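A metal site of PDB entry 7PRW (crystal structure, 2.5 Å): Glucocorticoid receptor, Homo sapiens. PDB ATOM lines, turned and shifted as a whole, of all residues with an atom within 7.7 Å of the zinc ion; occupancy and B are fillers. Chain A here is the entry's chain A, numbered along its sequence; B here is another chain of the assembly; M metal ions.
The side-chain sulfur (SG) of Cys 40 lies close to the guanidinium group (NE) of Arg 86, 3.5 Å away. N of Asp 42 sits close to SG of Cys 40 (3.7 Å). SG of Cys 54 is in hydrogen-bond range of N of Cys 57, 3.5 Å away. The side-chain sulfur (SG) of Cys 57 lies close to the guanidinium group (NH2) of Arg 93. SG of Cys 37 sits close to OG1 of Thr 53 (3.7 Å). The side-chain sulfur (SG) of Cys 54 sits at hydrogen-bond distance from the side-chain hydroxyl (OG) of Ser 56 (3.2 Å). O of Cys 40 sits at hydrogen-bond distance from N of Lys 83 (2.9 Å). SG of Cys 37 sits close to N of Cys 54, 3.6 Å away.
Within 4 Å of the zinc ion: Cys 37, Cys 40, Cys 54 and Cys 57. The nearest printed residue that does not touch the zinc ion is Ser 56 (4.2 Å).
SG of Cys 40 binds the zinc ion (2.2 Å). SG of Cys 57 binds the zinc ion (2.2 Å). The side-chain sulfur (SG) of Cys 37 binds the zinc ion, at 2.5 Å. Slightly farther from the zinc ion lies SG of Cys 54 (2.9 Å).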
ATOM      1  N   LEU A  36      34.846   0.125   8.875  1.00  0.00           N
ATOM      2  CA  LEU A  36      34.190  -1.167   9.093  1.00  0.00           C
ATOM      3  C   LEU A  36      33.795  -1.428  10.525  1.00  0.00           C
ATOM      4  O   LEU A  36      34.443  -0.942  11.435  1.00  0.00           O
ATOM      5  CB  LEU A  36      35.035  -2.327   8.546  1.00  0.00           C
ATOM      6  CG  LEU A  36      35.007  -2.644   7.029  1.00  0.00           C
ATOM      7  CD1 LEU A  36      35.185  -4.141   6.801  1.00  0.00           C
ATOM      8  CD2 LEU A  36      33.698  -2.197   6.348  1.00  0.00           C
ATOM      9  N   CYS A  37      32.717  -2.198  10.719  1.00  0.00           N
ATOM     10  CA  CYS A  37      32.222  -2.567  12.032  1.00  0.00           C
ATOM     11  C   CYS A  37      33.150  -3.620  12.631  1.00  0.00           C
ATOM     12  O   CYS A  37      33.255  -4.719  12.078  1.00  0.00           O
ATOM     13  CB  CYS A  37      30.783  -3.091  11.940  1.00  0.00           C
ATOM     14  SG  CYS A  37      30.120  -3.809  13.460  1.00  0.00           S
ATOM     15  N   LEU A  38      33.804  -3.290  13.757  1.00  0.00           N
ATOM     16  CA  LEU A  38      34.713  -4.200  14.459  1.00  0.00           C
ATOM     17  C   LEU A  38      34.057  -5.517  14.931  1.00  0.00           C
ATOM     18  O   LEU A  38      34.764  -6.373  15.457  1.00  0.00           O
ATOM     19  CB  LEU A  38      35.326  -3.508  15.675  1.00  0.00           C
ATOM     20  CG  LEU A  38      36.824  -3.261  15.597  1.00  0.00           C
ATOM     21  CD1 LEU A  38      37.137  -2.159  14.595  1.00  0.00           C
ATOM     22  CD2 LEU A  38      37.394  -2.929  16.974  1.00  0.00           C
ATOM     23  N   VAL A  39      32.715  -5.654  14.764  1.00  0.00           N
ATOM     24  CA  VAL A  39      31.912  -6.820  15.158  1.00  0.00           C
ATOM     25  C   VAL A  39      31.361  -7.631  13.947  1.00  0.00           C
ATOM     26  O   VAL A  39      31.679  -8.807  13.830  1.00  0.00           O
ATOM     27  CB  VAL A  39      30.789  -6.434  16.149  1.00  0.00           C
ATOM     28  CG1 VAL A  39      29.862  -7.613  16.432  1.00  0.00           C
ATOM     29  CG2 VAL A  39      31.364  -5.877  17.449  1.00  0.00           C
ATOM     30  N   CYS A  40      30.559  -7.018  13.066  1.00  0.00           N
ATOM     31  CA  CYS A  40      29.951  -7.733  11.933  1.00  0.00           C
ATOM     32  C   CYS A  40      30.568  -7.456  10.568  1.00  0.00           C
ATOM     33  O   CYS A  40      30.039  -7.945   9.577  1.00  0.00           O
ATOM     34  CB  CYS A  40      28.454  -7.466  11.904  1.00  0.00           C
ATOM     35  SG  CYS A  40      28.012  -5.761  11.480  1.00  0.00           S
ATOM     36  N   SER A  41      31.604  -6.621  10.507  1.00  0.00           N
ATOM     37  CA  SER A  41      32.322  -6.197   9.292  1.00  0.00           C
ATOM     38  C   SER A  41      31.477  -5.421   8.246  1.00  0.00           C
ATOM     39  O   SER A  41      32.005  -5.054   7.195  1.00  0.00           O
ATOM     40  CB  SER A  41      33.075  -7.360   8.647  1.00  0.00           C
ATOM     41  OG  SER A  41      34.447  -7.289   8.993  1.00  0.00           O
ATOM     42  N   ASP A  42      30.209  -5.086   8.549  1.00  0.00           N
ATOM     43  CA  ASP A  42      29.385  -4.226   7.693  1.00  0.00           C
ATOM     44  C   ASP A  42      29.871  -2.755   7.924  1.00  0.00           C
ATOM     45  O   ASP A  42      30.550  -2.486   8.903  1.00  0.00           O
ATOM     46  CB  ASP A  42      27.910  -4.381   8.103  1.00  0.00           C
ATOM     47  CG  ASP A  42      26.900  -3.591   7.289  1.00  0.00           C
ATOM     48  OD1 ASP A  42      27.263  -3.142   6.176  1.00  0.00           O
ATOM     49  OD2 ASP A  42      25.760  -3.434   7.754  1.00  0.00           O
ATOM     50  N   GLU A  43      29.558  -1.809   7.011  1.00  0.00           N
ATOM     51  CA  GLU A  43      30.005  -0.409   7.167  1.00  0.00           C
ATOM     52  C   GLU A  43      29.535   0.186   8.517  1.00  0.00           C
ATOM     53  O   GLU A  43      28.353   0.093   8.852  1.00  0.00           O
ATOM     54  CB  GLU A  43      29.552   0.462   5.983  1.00  0.00           C
ATOM     55  CG  GLU A  43      30.147   1.860   6.021  1.00  0.00           C
ATOM     56  CD  GLU A  43      29.634   2.830   4.967  1.00  0.00           C
ATOM     57  OE1 GLU A  43      28.612   2.507   4.318  1.00  0.00           O
ATOM     58  OE2 GLU A  43      30.249   3.905   4.798  1.00  0.00           O
ATOM     59  N   ALA A  44      30.487   0.728   9.296  1.00  0.00           N
ATOM     60  CA  ALA A  44      30.201   1.282  10.617  1.00  0.00           C
ATOM     61  C   ALA A  44      29.526   2.639  10.543  1.00  0.00           C
ATOM     62  O   ALA A  44      29.925   3.450   9.717  1.00  0.00           O
ATOM     63  CB  ALA A  44      31.486   1.391  11.429  1.00  0.00           C
ATOM     64  N   SER A  45      28.530   2.903  11.409  1.00  0.00           N
ATOM     65  CA  SER A  45      27.879   4.218  11.416  1.00  0.00           C
ATOM     66  C   SER A  45      28.612   5.273  12.293  1.00  0.00           C
ATOM     67  O   SER A  45      28.376   6.476  12.154  1.00  0.00           O
ATOM     68  CB  SER A  45      26.404   4.105  11.814  1.00  0.00           C
ATOM     69  OG  SER A  45      26.218   3.681  13.158  1.00  0.00           O
ATOM     70  N   LEU A  52      34.005   1.196  17.244  1.00  0.00           N
ATOM     71  CA  LEU A  52      33.596   1.467  15.862  1.00  0.00           C
ATOM     72  C   LEU A  52      32.636   0.378  15.471  1.00  0.00           C
ATOM     73  O   LEU A  52      33.038  -0.763  15.241  1.00  0.00           O
ATOM     74  CB  LEU A  52      34.812   1.409  14.934  1.00  0.00           C
ATOM     75  CG  LEU A  52      34.645   2.073  13.580  1.00  0.00           C
ATOM     76  CD1 LEU A  52      34.429   3.569  13.730  1.00  0.00           C
ATOM     77  CD2 LEU A  52      35.863   1.841  12.718  1.00  0.00           C
ATOM     78  N   THR A  53      31.363   0.700  15.539  1.00  0.00           N
ATOM     79  CA  THR A  53      30.318  -0.269  15.315  1.00  0.00           C
ATOM     80  C   THR A  53      29.257   0.280  14.387  1.00  0.00           C
ATOM     81  O   THR A  53      29.139   1.494  14.211  1.00  0.00           O
ATOM     82  CB  THR A  53      29.815  -0.704  16.702  1.00  0.00           C
ATOM     83  OG1 THR A  53      29.592  -2.094  16.711  1.00  0.00           O
ATOM     84  CG2 THR A  53      28.588   0.050  17.167  1.00  0.00           C
ATOM     85  N   CYS A  54      28.492  -0.612  13.763  1.00  0.00           N
ATOM     86  CA  CYS A  54      27.417  -0.192  12.876  1.00  0.00           C
ATOM     87  C   CYS A  54      26.116   0.083  13.687  1.00  0.00           C
ATOM     88  O   CYS A  54      26.114  -0.054  14.911  1.00  0.00           O
ATOM     89  CB  CYS A  54      27.218  -1.188  11.735  1.00  0.00           C
ATOM     90  SG  CYS A  54      25.934  -2.435  12.016  1.00  0.00           S
ATOM     91  N   GLY A  55      25.065   0.498  13.004  1.00  0.00           N
ATOM     92  CA  GLY A  55      23.787   0.771  13.644  1.00  0.00           C
ATOM     93  C   GLY A  55      23.126  -0.486  14.170  1.00  0.00           C
ATOM     94  O   GLY A  55      22.628  -0.490  15.302  1.00  0.00           O
ATOM     95  N   SER A  56      23.127  -1.585  13.378  1.00  0.00           N
ATOM     96  CA  SER A  56      22.494  -2.824  13.806  1.00  0.00           C
ATOM     97  C   SER A  56      23.181  -3.463  15.014  1.00  0.00           C
ATOM     98  O   SER A  56      22.527  -4.077  15.839  1.00  0.00           O
ATOM     99  CB  SER A  56      22.429  -3.826  12.661  1.00  0.00           C
ATOM    100  OG  SER A  56      23.620  -4.587  12.536  1.00  0.00           O
ATOM    101  N   CYS A  57      24.511  -3.366  15.050  1.00  0.00           N
ATOM    102  CA  CYS A  57      25.325  -3.915  16.127  1.00  0.00           C
ATOM    103  C   CYS A  57      25.215  -3.110  17.397  1.00  0.00           C
ATOM    104  O   CYS A  57      25.386  -3.652  18.469  1.00  0.00           O
ATOM    105  CB  CYS A  57      26.777  -4.031  15.678  1.00  0.00           C
ATOM    106  SG  CYS A  57      27.181  -5.587  14.859  1.00  0.00           S
ATOM    107  N   LYS A  58      24.987  -1.802  17.280  1.00  0.00           N
ATOM    108  CA  LYS A  58      24.863  -0.908  18.422  1.00  0.00           C
ATOM    109  C   LYS A  58      23.610  -1.288  19.215  1.00  0.00           C
ATOM    110  O   LYS A  58      23.694  -1.537  20.415  1.00  0.00           O
ATOM    111  CB  LYS A  58      24.820   0.571  17.936  1.00  0.00           C
ATOM    112  CG  LYS A  58      23.966   1.543  18.776  1.00  0.00           C
ATOM    113  CD  LYS A  58      23.723   2.865  18.043  1.00  0.00           C
ATOM    114  CE  LYS A  58      23.183   3.945  18.953  1.00  0.00           C
ATOM    115  NZ  LYS A  58      21.981   3.502  19.684  1.00  0.00           N
ATOM    116  N   PHE A  60      21.751  -4.017  18.975  1.00  0.00           N
ATOM    117  CA  PHE A  60      21.827  -5.399  19.424  1.00  0.00           C
ATOM    118  C   PHE A  60      22.534  -5.430  20.801  1.00  0.00           C
ATOM    119  O   PHE A  60      22.074  -6.098  21.702  1.00  0.00           O
ATOM    120  CB  PHE A  60      22.584  -6.282  18.430  1.00  0.00           C
ATOM    121  CG  PHE A  60      22.825  -7.678  18.966  1.00  0.00           C
ATOM    122  CD1 PHE A  60      21.858  -8.659  18.852  1.00  0.00           C
ATOM    123  CD2 PHE A  60      23.977  -7.982  19.660  1.00  0.00           C
ATOM    124  CE1 PHE A  60      22.058  -9.914  19.385  1.00  0.00           C
ATOM    125  CE2 PHE A  60      24.165  -9.241  20.214  1.00  0.00           C
ATOM    126  CZ  PHE A  60      23.214 -10.194  20.067  1.00  0.00           C
ATOM    127  N   ILE A  81      30.953 -14.081  12.912  1.00  0.00           N
ATOM    128  CA  ILE A  81      30.015 -12.973  12.898  1.00  0.00           C
ATOM    129  C   ILE A  81      30.342 -12.032  11.721  1.00  0.00           C
ATOM    130  O   ILE A  81      31.418 -11.409  11.679  1.00  0.00           O
ATOM    131  CB  ILE A  81      29.883 -12.249  14.255  1.00  0.00           C
ATOM    132  CG1 ILE A  81      29.713 -13.261  15.403  1.00  0.00           C
ATOM    133  CG2 ILE A  81      28.731 -11.252  14.211  1.00  0.00           C
ATOM    134  CD1 ILE A  81      28.489 -14.141  15.316  1.00  0.00           C
ATOM    135  N   ASP A  82      29.451 -11.991  10.739  1.00  0.00           N
ATOM    136  CA  ASP A  82      29.569 -11.111   9.584  1.00  0.00           C
ATOM    137  C   ASP A  82      28.185 -10.545   9.183  1.00  0.00           C
ATOM    138  O   ASP A  82      27.185 -10.916   9.814  1.00  0.00           O
ATOM    139  CB  ASP A  82      30.352 -11.772   8.420  1.00  0.00           C
ATOM    140  CG  ASP A  82      29.703 -12.960   7.717  1.00  0.00           C
ATOM    141  OD1 ASP A  82      28.577 -13.366   8.129  1.00  0.00           O
ATOM    142  OD2 ASP A  82      30.307 -13.479   6.751  1.00  0.00           O
ATOM    143  N   LYS A  83      28.111  -9.622   8.199  1.00  0.00           N
ATOM    144  CA  LYS A  83      26.838  -9.024   7.783  1.00  0.00           C
ATOM    145  C   LYS A  83      25.705 -10.061   7.556  1.00  0.00           C
ATOM    146  O   LYS A  83      24.569  -9.880   8.022  1.00  0.00           O
ATOM    147  CB  LYS A  83      27.055  -8.126   6.534  1.00  0.00           C
ATOM    148  CG  LYS A  83      25.758  -7.704   5.809  1.00  0.00           C
ATOM    149  CD  LYS A  83      25.848  -6.311   5.208  1.00  0.00           C
ATOM    150  CE  LYS A  83      24.507  -5.812   4.701  1.00  0.00           C
ATOM    151  NZ  LYS A  83      24.615  -4.424   4.128  1.00  0.00           N
ATOM    152  N   ARG A  86      25.041 -12.258  11.222  1.00  0.00           N
ATOM    153  CA  ARG A  86      24.919 -11.599  12.532  1.00  0.00           C
ATOM    154  C   ARG A  86      23.592 -11.944  13.230  1.00  0.00           C
ATOM    155  O   ARG A  86      23.502 -11.950  14.466  1.00  0.00           O
ATOM    156  CB  ARG A  86      25.196 -10.090  12.473  1.00  0.00           C
ATOM    157  CG  ARG A  86      24.613  -9.358  11.276  1.00  0.00           C
ATOM    158  CD  ARG A  86      24.551  -7.896  11.626  1.00  0.00           C
ATOM    159  NE  ARG A  86      24.883  -7.006  10.523  1.00  0.00           N
ATOM    160  CZ  ARG A  86      24.005  -6.269   9.851  1.00  0.00           C
ATOM    161  NH1 ARG A  86      24.404  -5.466   8.883  1.00  0.00           N
ATOM    162  NH2 ARG A  86      22.708  -6.316  10.165  1.00  0.00           N
ATOM    163  N   ARG A  93      27.503 -13.171  18.932  1.00  0.00           N
ATOM    164  CA  ARG A  93      27.506 -11.759  18.582  1.00  0.00           C
ATOM    165  C   ARG A  93      27.627 -10.974  19.866  1.00  0.00           C
ATOM    166  O   ARG A  93      28.459 -10.082  19.907  1.00  0.00           O
ATOM    167  CB  ARG A  93      26.248 -11.374  17.825  1.00  0.00           C
ATOM    168  CG  ARG A  93      26.264  -9.954  17.319  1.00  0.00           C
ATOM    169  CD  ARG A  93      24.966  -9.688  16.633  1.00  0.00           C
ATOM    170  NE  ARG A  93      24.895  -8.426  15.913  1.00  0.00           N
ATOM    171  CZ  ARG A  93      23.822  -8.003  15.239  1.00  0.00           C
ATOM    172  NH1 ARG A  93      22.728  -8.748  15.208  1.00  0.00           N
ATOM    173  NH2 ARG A  93      23.834  -6.829  14.624  1.00  0.00           N
ATOM    174  N   CYS A  97      30.857  -8.446  20.866  1.00  0.00           N
ATOM    175  CA  CYS A  97      30.728  -7.050  21.305  1.00  0.00           C
ATOM    176  C   CYS A  97      31.626  -6.826  22.531  1.00  0.00           C
ATOM    177  O   CYS A  97      32.205  -5.755  22.675  1.00  0.00           O
ATOM    178  CB  CYS A  97      29.275  -6.700  21.614  1.00  0.00           C
ATOM    179  SG  CYS A  97      28.165  -6.716  20.180  1.00  0.00           S
ATOM    180  P    DG B  15      20.391  -7.310  12.438  1.00  0.00           P
ATOM    181  OP1  DG B  15      21.193  -7.909  11.355  1.00  0.00           O
ATOM    182  OP2  DG B  15      21.011  -7.011  13.747  1.00  0.00           O
ATOM    183  O5'  DG B  15      19.717  -5.977  11.901  1.00  0.00           O
ATOM    184  C5'  DG B  15      19.046  -5.974  10.670  1.00  0.00           C
ATOM    185  C4'  DG B  15      18.460  -4.601  10.432  1.00  0.00           C
ATOM    186  O4'  DG B  15      17.458  -4.336  11.440  1.00  0.00           O
ATOM    187  C3'  DG B  15      19.466  -3.416  10.502  1.00  0.00           C
ATOM    188  O3'  DG B  15      19.326  -2.603   9.328  1.00  0.00           O
ATOM    189  C2'  DG B  15      19.032  -2.655  11.764  1.00  0.00           C
ATOM    190  C1'  DG B  15      17.555  -2.977  11.793  1.00  0.00           C
ATOM    191  N9   DG B  15      16.912  -2.758  13.072  1.00  0.00           N
ATOM    192  C8   DG B  15      17.164  -3.401  14.269  1.00  0.00           C
ATOM    193  N7   DG B  15      16.411  -2.974  15.246  1.00  0.00           N
ATOM    194  C5   DG B  15      15.622  -2.004  14.666  1.00  0.00           C
ATOM    195  C6   DG B  15      14.602  -1.193  15.230  1.00  0.00           C
ATOM    196  O6   DG B  15      14.193  -1.161  16.398  1.00  0.00           O
ATOM    197  N1   DG B  15      14.050  -0.332  14.282  1.00  0.00           N
ATOM    198  C2   DG B  15      14.442  -0.256  12.959  1.00  0.00           C
ATOM    199  N2   DG B  15      13.785   0.603  12.183  1.00  0.00           N
ATOM    200  N3   DG B  15      15.348  -1.054  12.420  1.00  0.00           N
ATOM    201  C4   DG B  15      15.926  -1.855  13.336  1.00  0.00           C
HETATM  202 ZN    ZN M   1      27.740  -4.358  13.100  1.00  0.00          ZN
